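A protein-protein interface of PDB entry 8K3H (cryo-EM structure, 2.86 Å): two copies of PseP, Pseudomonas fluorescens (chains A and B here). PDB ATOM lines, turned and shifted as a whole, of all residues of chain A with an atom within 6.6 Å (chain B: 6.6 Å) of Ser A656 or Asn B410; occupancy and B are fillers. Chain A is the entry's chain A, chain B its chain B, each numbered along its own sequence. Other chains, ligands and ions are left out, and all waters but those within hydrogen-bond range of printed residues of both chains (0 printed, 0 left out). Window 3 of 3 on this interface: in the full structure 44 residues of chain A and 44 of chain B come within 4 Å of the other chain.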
ATOM      1  N   SER A 463      31.679  20.104   3.350  1.00  0.00           N
ATOM      2  CA  SER A 463      30.533  20.612   2.602  1.00  0.00           C
ATOM      3  C   SER A 463      30.560  22.129   2.471  1.00  0.00           C
ATOM      4  O   SER A 463      30.062  22.671   1.479  1.00  0.00           O
ATOM      5  CB  SER A 463      29.233  20.164   3.269  1.00  0.00           C
ATOM      6  OG  SER A 463      29.115  18.754   3.252  1.00  0.00           O
ATOM      7  N   TYR A 651      23.303  25.750   6.779  1.00  0.00           N
ATOM      8  CA  TYR A 651      23.547  25.512   5.362  1.00  0.00           C
ATOM      9  C   TYR A 651      24.467  24.322   5.121  1.00  0.00           C
ATOM     10  O   TYR A 651      24.518  23.814   3.996  1.00  0.00           O
ATOM     11  CB  TYR A 651      24.131  26.772   4.719  1.00  0.00           C
ATOM     12  CG  TYR A 651      24.291  26.689   3.217  1.00  0.00           C
ATOM     13  CD1 TYR A 651      23.206  26.876   2.371  1.00  0.00           C
ATOM     14  CD2 TYR A 651      25.530  26.429   2.645  1.00  0.00           C
ATOM     15  CE1 TYR A 651      23.348  26.802   1.000  1.00  0.00           C
ATOM     16  CE2 TYR A 651      25.682  26.352   1.276  1.00  0.00           C
ATOM     17  CZ  TYR A 651      24.588  26.540   0.458  1.00  0.00           C
ATOM     18  OH  TYR A 651      24.737  26.465  -0.908  1.00  0.00           O
ATOM     19  N   TYR A 652      25.191  23.865   6.146  1.00  0.00           N
ATOM     20  CA  TYR A 652      26.071  22.713   5.976  1.00  0.00           C
ATOM     21  C   TYR A 652      25.281  21.470   5.586  1.00  0.00           C
ATOM     22  O   TYR A 652      25.706  20.704   4.713  1.00  0.00           O
ATOM     23  CB  TYR A 652      26.867  22.467   7.260  1.00  0.00           C
ATOM     24  CG  TYR A 652      27.782  21.259   7.210  1.00  0.00           C
ATOM     25  CD1 TYR A 652      27.314  19.988   7.524  1.00  0.00           C
ATOM     26  CD2 TYR A 652      29.116  21.391   6.849  1.00  0.00           C
ATOM     27  CE1 TYR A 652      28.145  18.888   7.475  1.00  0.00           C
ATOM     28  CE2 TYR A 652      29.955  20.296   6.799  1.00  0.00           C
ATOM     29  CZ  TYR A 652      29.465  19.048   7.113  1.00  0.00           C
ATOM     30  OH  TYR A 652      30.298  17.954   7.066  1.00  0.00           O
ATOM     31  N   GLU A 653      24.130  21.250   6.225  1.00  0.00           N
ATOM     32  CA  GLU A 653      23.321  20.077   5.909  1.00  0.00           C
ATOM     33  C   GLU A 653      22.742  20.167   4.503  1.00  0.00           C
ATOM     34  O   GLU A 653      22.628  19.151   3.807  1.00  0.00           O
ATOM     35  CB  GLU A 653      22.207  19.914   6.941  1.00  0.00           C
ATOM     36  N   PHE A 654      22.363  21.371   4.069  1.00  0.00           N
ATOM     37  CA  PHE A 654      21.825  21.537   2.722  1.00  0.00           C
ATOM     38  C   PHE A 654      22.890  21.258   1.668  1.00  0.00           C
ATOM     39  O   PHE A 654      22.637  20.548   0.689  1.00  0.00           O
ATOM     40  CB  PHE A 654      21.251  22.946   2.556  1.00  0.00           C
ATOM     41  CG  PHE A 654      20.781  23.252   1.159  1.00  0.00           C
ATOM     42  CD1 PHE A 654      21.643  23.800   0.223  1.00  0.00           C
ATOM     43  CD2 PHE A 654      19.476  22.987   0.784  1.00  0.00           C
ATOM     44  CE1 PHE A 654      21.211  24.074  -1.058  1.00  0.00           C
ATOM     45  CE2 PHE A 654      19.039  23.262  -0.496  1.00  0.00           C
ATOM     46  CZ  PHE A 654      19.908  23.806  -1.418  1.00  0.00           C
ATOM     47  N   ALA A 655      24.091  21.814   1.854  1.00  0.00           N
ATOM     48  CA  ALA A 655      25.151  21.642   0.867  1.00  0.00           C
ATOM     49  C   ALA A 655      25.588  20.187   0.753  1.00  0.00           C
ATOM     50  O   ALA A 655      25.916  19.723  -0.345  1.00  0.00           O
ATOM     51  CB  ALA A 655      26.345  22.528   1.218  1.00  0.00           C
ATOM     52  N   SER A 656      25.606  19.458   1.870  1.00  0.00           N
ATOM     53  CA  SER A 656      25.994  18.052   1.832  1.00  0.00           C
ATOM     54  C   SER A 656      25.008  17.226   1.014  1.00  0.00           C
ATOM     55  O   SER A 656      25.410  16.320   0.277  1.00  0.00           O
ATOM     56  CB  SER A 656      26.103  17.502   3.254  1.00  0.00           C
ATOM     57  OG  SER A 656      26.523  16.149   3.244  1.00  0.00           O
ATOM     58  N   THR A 657      23.714  17.521   1.136  1.00  0.00           N
ATOM     59  CA  THR A 657      22.705  16.764   0.403  1.00  0.00           C
ATOM     60  C   THR A 657      22.583  17.232  -1.042  1.00  0.00           C
ATOM     61  O   THR A 657      22.465  16.407  -1.956  1.00  0.00           O
ATOM     62  CB  THR A 657      21.353  16.878   1.106  1.00  0.00           C
ATOM     63  OG1 THR A 657      21.488  16.482   2.475  1.00  0.00           O
ATOM     64  CG2 THR A 657      20.324  15.993   0.426  1.00  0.00           C
ATOM     65  N   SER A 658      22.608  18.547  -1.268  1.00  0.00           N
ATOM     66  CA  SER A 658      22.346  19.082  -2.601  1.00  0.00           C
ATOM     67  C   SER A 658      23.465  18.729  -3.575  1.00  0.00           C
ATOM     68  O   SER A 658      23.209  18.246  -4.683  1.00  0.00           O
ATOM     69  CB  SER A 658      22.151  20.597  -2.524  1.00  0.00           C
ATOM     70  OG  SER A 658      21.865  21.139  -3.802  1.00  0.00           O
ATOM     71  N   TYR A 659      24.717  18.972  -3.187  1.00  0.00           N
ATOM     72  CA  TYR A 659      25.846  18.698  -4.064  1.00  0.00           C
ATOM     73  C   TYR A 659      27.044  18.071  -3.368  1.00  0.00           C
ATOM     74  O   TYR A 659      28.034  17.775  -4.045  1.00  0.00           O
ATOM     75  CB  TYR A 659      26.299  19.983  -4.780  1.00  0.00           C
ATOM     76  CG  TYR A 659      26.472  21.188  -3.880  1.00  0.00           C
ATOM     77  CD1 TYR A 659      25.393  22.000  -3.560  1.00  0.00           C
ATOM     78  CD2 TYR A 659      27.717  21.522  -3.367  1.00  0.00           C
ATOM     79  CE1 TYR A 659      25.547  23.102  -2.743  1.00  0.00           C
ATOM     80  CE2 TYR A 659      27.881  22.623  -2.551  1.00  0.00           C
ATOM     81  CZ  TYR A 659      26.793  23.409  -2.243  1.00  0.00           C
ATOM     82  OH  TYR A 659      26.951  24.507  -1.430  1.00  0.00           O
ATOM     83  N   GLY A 660      26.994  17.858  -2.052  1.00  0.00           N
ATOM     84  CA  GLY A 660      28.061  17.231  -1.312  1.00  0.00           C
ATOM     85  C   GLY A 660      29.139  18.184  -0.832  1.00  0.00           C
ATOM     86  O   GLY A 660      29.729  17.952   0.229  1.00  0.00           O
ATOM     87  N   GLY A 661      29.415  19.240  -1.590  1.00  0.00           N
ATOM     88  CA  GLY A 661      30.419  20.204  -1.212  1.00  0.00           C
ATOM     89  C   GLY A 661      30.989  20.925  -2.414  1.00  0.00           C
ATOM     90  O   GLY A 661      30.721  20.568  -3.564  1.00  0.00           O
ATOM     91  N   ARG B 357      18.084  10.762  15.934  1.00  0.00           N
ATOM     92  CA  ARG B 357      19.538  10.635  15.912  1.00  0.00           C
ATOM     93  C   ARG B 357      20.114  10.617  17.323  1.00  0.00           C
ATOM     94  O   ARG B 357      21.039   9.850  17.614  1.00  0.00           O
ATOM     95  CB  ARG B 357      20.152  11.772  15.096  1.00  0.00           C
ATOM     96  CG  ARG B 357      21.671  11.792  15.109  1.00  0.00           C
ATOM     97  CD  ARG B 357      22.210  13.196  14.912  1.00  0.00           C
ATOM     98  NE  ARG B 357      22.478  13.866  16.178  1.00  0.00           N
ATOM     99  CZ  ARG B 357      23.253  14.934  16.309  1.00  0.00           C
ATOM    100  NH1 ARG B 357      23.855  15.483  15.268  1.00  0.00           N
ATOM    101  NH2 ARG B 357      23.427  15.464  17.516  1.00  0.00           N
ATOM    102  N   VAL B 405      19.012   8.853   9.321  1.00  0.00           N
ATOM    103  CA  VAL B 405      20.233   8.283   8.761  1.00  0.00           C
ATOM    104  C   VAL B 405      21.145   9.386   8.238  1.00  0.00           C
ATOM    105  O   VAL B 405      22.372   9.319   8.383  1.00  0.00           O
ATOM    106  CB  VAL B 405      19.888   7.255   7.668  1.00  0.00           C
ATOM    107  CG1 VAL B 405      21.139   6.824   6.917  1.00  0.00           C
ATOM    108  CG2 VAL B 405      19.191   6.051   8.278  1.00  0.00           C
ATOM    109  N   LYS B 406      20.563  10.426   7.635  1.00  0.00           N
ATOM    110  CA  LYS B 406      21.372  11.529   7.127  1.00  0.00           C
ATOM    111  C   LYS B 406      21.988  12.343   8.259  1.00  0.00           C
ATOM    112  O   LYS B 406      23.110  12.844   8.118  1.00  0.00           O
ATOM    113  CB  LYS B 406      20.532  12.424   6.218  1.00  0.00           C
ATOM    114  CG  LYS B 406      21.323  13.532   5.543  1.00  0.00           C
ATOM    115  CD  LYS B 406      22.416  12.959   4.658  1.00  0.00           C
ATOM    116  CE  LYS B 406      23.079  14.037   3.821  1.00  0.00           C
ATOM    117  NZ  LYS B 406      23.853  14.993   4.656  1.00  0.00           N
ATOM    118  N   GLU B 407      21.279  12.493   9.381  1.00  0.00           N
ATOM    119  CA  GLU B 407      21.876  13.156  10.536  1.00  0.00           C
ATOM    120  C   GLU B 407      23.007  12.322  11.125  1.00  0.00           C
ATOM    121  O   GLU B 407      24.043  12.865  11.524  1.00  0.00           O
ATOM    122  CB  GLU B 407      20.811  13.448  11.596  1.00  0.00           C
ATOM    123  CG  GLU B 407      19.709  14.407  11.154  1.00  0.00           C
ATOM    124  CD  GLU B 407      20.186  15.838  10.958  1.00  0.00           C
ATOM    125  OE1 GLU B 407      21.386  16.119  11.164  1.00  0.00           O
ATOM    126  OE2 GLU B 407      19.349  16.692  10.594  1.00  0.00           O
ATOM    127  N   LEU B 408      22.824  11.000  11.193  1.00  0.00           N
ATOM    128  CA  LEU B 408      23.927  10.125  11.575  1.00  0.00           C
ATOM    129  C   LEU B 408      25.058  10.192  10.559  1.00  0.00           C
ATOM    130  O   LEU B 408      26.232  10.059  10.923  1.00  0.00           O
ATOM    131  CB  LEU B 408      23.434   8.686  11.730  1.00  0.00           C
ATOM    132  CG  LEU B 408      22.417   8.414  12.839  1.00  0.00           C
ATOM    133  CD1 LEU B 408      21.751   7.063  12.634  1.00  0.00           C
ATOM    134  CD2 LEU B 408      23.081   8.484  14.205  1.00  0.00           C
ATOM    135  N   PHE B 409      24.722  10.388   9.282  1.00  0.00           N
ATOM    136  CA  PHE B 409      25.743  10.606   8.264  1.00  0.00           C
ATOM    137  C   PHE B 409      26.531  11.879   8.544  1.00  0.00           C
ATOM    138  O   PHE B 409      27.760  11.901   8.410  1.00  0.00           O
ATOM    139  CB  PHE B 409      25.083  10.660   6.884  1.00  0.00           C
ATOM    140  CG  PHE B 409      26.052  10.756   5.740  1.00  0.00           C
ATOM    141  CD1 PHE B 409      26.556   9.613   5.144  1.00  0.00           C
ATOM    142  CD2 PHE B 409      26.434  11.989   5.239  1.00  0.00           C
ATOM    143  CE1 PHE B 409      27.437   9.699   4.084  1.00  0.00           C
ATOM    144  CE2 PHE B 409      27.315  12.081   4.180  1.00  0.00           C
ATOM    145  CZ  PHE B 409      27.815  10.934   3.601  1.00  0.00           C
ATOM    146  N   ASN B 410      25.839  12.951   8.937  1.00  0.00           N
ATOM    147  CA  ASN B 410      26.524  14.200   9.257  1.00  0.00           C
ATOM    148  C   ASN B 410      27.322  14.080  10.549  1.00  0.00           C
ATOM    149  O   ASN B 410      28.453  14.573  10.633  1.00  0.00           O
ATOM    150  CB  ASN B 410      25.513  15.341   9.358  1.00  0.00           C
ATOM    151  CG  ASN B 410      25.003  15.788   8.004  1.00  0.00           C
ATOM    152  OD1 ASN B 410      25.690  15.648   6.993  1.00  0.00           O
ATOM    153  ND2 ASN B 410      23.792  16.330   7.978  1.00  0.00           N
ATOM    154  N   ALA B 411      26.753  13.428  11.566  1.00  0.00           N
ATOM    155  CA  ALA B 411      27.452  13.286  12.838  1.00  0.00           C
ATOM    156  C   ALA B 411      28.684  12.402  12.711  1.00  0.00           C
ATOM    157  O   ALA B 411      29.648  12.574  13.464  1.00  0.00           O
ATOM    158  CB  ALA B 411      26.505  12.723  13.898  1.00  0.00           C
ATOM    159  N   PHE B 412      28.667  11.447  11.780  1.00  0.00           N
ATOM    160  CA  PHE B 412      29.815  10.563  11.606  1.00  0.00           C
ATOM    161  C   PHE B 412      31.053  11.335  11.164  1.00  0.00           C
ATOM    162  O   PHE B 412      32.154  11.100  11.675  1.00  0.00           O
ATOM    163  CB  PHE B 412      29.473   9.466  10.596  1.00  0.00           C
ATOM    164  CG  PHE B 412      30.624   8.557  10.268  1.00  0.00           C
ATOM    165  CD1 PHE B 412      30.967   7.517  11.114  1.00  0.00           C
ATOM    166  CD2 PHE B 412      31.352   8.733   9.102  1.00  0.00           C
ATOM    167  CE1 PHE B 412      32.021   6.679  10.810  1.00  0.00           C
ATOM    168  CE2 PHE B 412      32.407   7.897   8.796  1.00  0.00           C
ATOM    169  CZ  PHE B 412      32.741   6.868   9.650  1.00  0.00           C
ATOM    170  N   PHE B 413      30.894  12.261  10.219  1.00  0.00           N
ATOM    171  CA  PHE B 413      32.051  12.926   9.626  1.00  0.00           C
ATOM    172  C   PHE B 413      32.529  14.107  10.466  1.00  0.00           C
ATOM    173  O   PHE B 413      33.659  14.108  10.965  1.00  0.00           O
ATOM    174  CB  PHE B 413      31.719  13.374   8.201  1.00  0.00           C
ATOM    175  CG  PHE B 413      31.648  12.245   7.216  1.00  0.00           C
ATOM    176  CD1 PHE B 413      32.802  11.612   6.785  1.00  0.00           C
ATOM    177  CD2 PHE B 413      30.430  11.808   6.727  1.00  0.00           C
ATOM    178  CE1 PHE B 413      32.742  10.570   5.881  1.00  0.00           C
ATOM    179  CE2 PHE B 413      30.364  10.766   5.825  1.00  0.00           C
ATOM    180  CZ  PHE B 413      31.521  10.146   5.401  1.00  0.00           C
ATOM    181  N   ARG B 414      31.681  15.124  10.635  1.00  0.00           N
ATOM    182  CA  ARG B 414      32.132  16.360  11.265  1.00  0.00           C
ATOM    183  C   ARG B 414      32.120  16.302  12.785  1.00  0.00           C
ATOM    184  O   ARG B 414      32.729  17.166  13.426  1.00  0.00           O
ATOM    185  CB  ARG B 414      31.274  17.542  10.804  1.00  0.00           C
ATOM    186  CG  ARG B 414      29.796  17.400  11.118  1.00  0.00           C
ATOM    187  CD  ARG B 414      29.055  18.710  10.902  1.00  0.00           C
ATOM    188  NE  ARG B 414      27.608  18.522  10.898  1.00  0.00           N
ATOM    189  CZ  ARG B 414      26.867  18.372  11.987  1.00  0.00           C
ATOM    190  NH1 ARG B 414      27.404  18.382  13.196  1.00  0.00           N
ATOM    191  NH2 ARG B 414      25.554  18.206  11.859  1.00  0.00           N
ATOM    192  N   ASP B 415      31.448  15.319  13.381  1.00  0.00           N
ATOM    193  CA  ASP B 415      31.347  15.250  14.832  1.00  0.00           C
ATOM    194  C   ASP B 415      32.135  14.101  15.444  1.00  0.00           C
ATOM    195  O   ASP B 415      32.567  14.214  16.595  1.00  0.00           O
ATOM    196  CB  ASP B 415      29.879  15.130  15.258  1.00  0.00           C
ATOM    197  CG  ASP B 415      29.194  16.476  15.371  1.00  0.00           C
ATOM    198  OD1 ASP B 415      29.618  17.422  14.675  1.00  0.00           O
ATOM    199  OD2 ASP B 415      28.228  16.587  16.155  1.00  0.00           O
ATOM    200  N   ASP B 416      32.330  13.000  14.719  1.00  0.00           N
ATOM    201  CA  ASP B 416      32.990  11.825  15.272  1.00  0.00           C
ATOM    202  C   ASP B 416      34.328  11.528  14.608  1.00  0.00           C
ATOM    203  O   ASP B 416      35.354  11.467  15.291  1.00  0.00           O
ATOM    204  CB  ASP B 416      32.060  10.609  15.160  1.00  0.00           C
ATOM    205  CG  ASP B 416      31.000  10.585  16.241  1.00  0.00           C
ATOM    206  OD1 ASP B 416      30.591  11.672  16.699  1.00  0.00           O
ATOM    207  OD2 ASP B 416      30.573   9.479  16.632  1.00  0.00           O
ATOM    208  N   THR B 498      25.996  13.326  -7.150  1.00  0.00           N
ATOM    209  CA  THR B 498      25.176  13.859  -6.066  1.00  0.00           C
ATOM    210  C   THR B 498      24.378  15.069  -6.526  1.00  0.00           C
ATOM    211  O   THR B 498      23.191  15.200  -6.207  1.00  0.00           O
ATOM    212  CB  THR B 498      26.051  14.222  -4.867  1.00  0.00           C
ATOM    213  OG1 THR B 498      26.919  13.125  -4.555  1.00  0.00           O
ATOM    214  CG2 THR B 498      25.192  14.542  -3.654  1.00  0.00           C
ATOM    215  N   TYR B 525      22.891   5.671  -0.907  1.00  0.00           N
ATOM    216  CA  TYR B 525      23.706   6.767  -0.402  1.00  0.00           C
ATOM    217  C   TYR B 525      22.804   7.797   0.266  1.00  0.00           C
ATOM    218  O   TYR B 525      21.889   8.316  -0.388  1.00  0.00           O
ATOM    219  CB  TYR B 525      24.489   7.405  -1.536  1.00  0.00           C
ATOM    220  CG  TYR B 525      25.656   8.265  -1.106  1.00  0.00           C
ATOM    221  CD1 TYR B 525      26.462   7.894  -0.039  1.00  0.00           C
ATOM    222  CD2 TYR B 525      25.964   9.436  -1.784  1.00  0.00           C
ATOM    223  CE1 TYR B 525      27.533   8.675   0.350  1.00  0.00           C
ATOM    224  CE2 TYR B 525      27.033  10.222  -1.403  1.00  0.00           C
ATOM    225  CZ  TYR B 525      27.814   9.836  -0.336  1.00  0.00           C
ATOM    226  OH  TYR B 525      28.880  10.617   0.047  1.00  0.00           O
ATOM    227  N   PRO B 527      22.979  10.973   1.076  1.00  0.00           N
ATOM    228  CA  PRO B 527      22.756  12.243   0.361  1.00  0.00           C
ATOM    229  C   PRO B 527      21.786  12.126  -0.803  1.00  0.00           C
ATOM    230  O   PRO B 527      21.004  13.053  -1.046  1.00  0.00           O
ATOM    231  CB  PRO B 527      24.165  12.625  -0.107  1.00  0.00           C
ATOM    232  CG  PRO B 527      25.043  12.057   0.922  1.00  0.00           C
ATOM    233  CD  PRO B 527      24.424  10.733   1.260  1.00  0.00           C
ATOM    234  N   TRP B 534      13.421  15.302  -0.058  1.00  0.00           N
ATOM    235  CA  TRP B 534      13.132  16.730  -0.018  1.00  0.00           C
ATOM    236  C   TRP B 534      11.891  17.067  -0.834  1.00  0.00           C
ATOM    237  O   TRP B 534      11.068  17.890  -0.418  1.00  0.00           O
ATOM    238  CB  TRP B 534      14.332  17.519  -0.538  1.00  0.00           C
ATOM    239  CG  TRP B 534      15.356  17.842   0.497  1.00  0.00           C
ATOM    240  CD1 TRP B 534      15.265  17.626   1.840  1.00  0.00           C
ATOM    241  CD2 TRP B 534      16.635  18.443   0.273  1.00  0.00           C
ATOM    242  NE1 TRP B 534      16.408  18.058   2.466  1.00  0.00           N
ATOM    243  CE2 TRP B 534      17.266  18.564   1.525  1.00  0.00           C
ATOM    244  CE3 TRP B 534      17.308  18.891  -0.868  1.00  0.00           C
ATOM    245  CZ2 TRP B 534      18.536  19.115   1.669  1.00  0.00           C
ATOM    246  CZ3 TRP B 534      18.567  19.439  -0.723  1.00  0.00           C
ATOM    247  CH2 TRP B 534      19.168  19.546   0.537  1.00  0.00           C
ATOM    248  N   LEU B 781      24.939   3.786   8.071  1.00  0.00           N
ATOM    249  CA  LEU B 781      25.128   4.849   7.095  1.00  0.00           C
ATOM    250  C   LEU B 781      24.874   4.385   5.668  1.00  0.00           C
ATOM    251  O   LEU B 781      24.860   5.218   4.756  1.00  0.00           O
ATOM    252  CB  LEU B 781      26.542   5.417   7.213  1.00  0.00           C
ATOM    253  CG  LEU B 781      26.896   6.071   8.548  1.00  0.00           C
ATOM    254  CD1 LEU B 781      28.204   6.828   8.431  1.00  0.00           C
ATOM    255  CD2 LEU B 781      25.780   6.988   9.015  1.00  0.00           C
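The side-chain hydroxyl of Ser A656 sits at hydrogen-bond distance from the side-chain amino group of Lys B406, 3.2 Å away.
The backbone carbonyl oxygen (O) of Thr B498 sits close to the backbone carbonyl oxygen (O) of Ser A658 (3.4 Å).
The side-chain hydroxyl of Tyr A659 sits at hydrogen-bond distance from the side-chain hydroxyl of Tyr A651.
The side-chain hydroxyl (OG1) of Thr A657 is in hydrogen-bond range of the backbone carbonyl oxygen (O) of Glu A653 (3.2 Å).
NZ of Lys B406 is in hydrogen-bond range of OD1 of Asn B410, 3.0 Å away.
The guanidinium group of Arg B414 is in salt-bridge range of the side-chain carboxylate of Asp B415 (2.8 Å).
Among the printed residues, pairs that only touch across the chains: Thr A657 with Lys B406, Thr A657 with Pro B527, Phe A654 with Trp B534, Tyr A652 with Arg B414, Thr A657 with Trp B534, Thr A657 with Thr B498, Ser A656 with Asn B410, Ser A656 with Pro B527 and Tyr A659 with Thr B498.
Of the printed residues of chain B, Ser A656 touches Lys B406, Asn B410 and Pro B527.
Of the printed residues of chain A, Asn B410 touches Ser A656 (3.9 Å).
Printed residues of chain B within 4 Å of Tyr A652: Arg B414.
Of the printed residues of chain B, Ser A658 touches Thr B498.
Printed residues of chain B within 4 Å of Phe A654: Trp B534 (3.5 Å).
Printed residues of chain A within 4 Å of Arg B414: Tyr A652.
Ala A655 touches none of the printed residues of chain B.
Phe B413 touches none of the printed residues of chain A.
Hydrophobic or aromatic side chains of chain B within 4 Å of the printed part of chain A: Pro B527 and Trp B534.
Of the 12 printed residues of chain A, 6 touch a printed residue of chain B.
No position is printed for both chains.
Of the 11 pairs that touch across the chains among the printed residues, none has its exchanged pair printed and touching as well.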
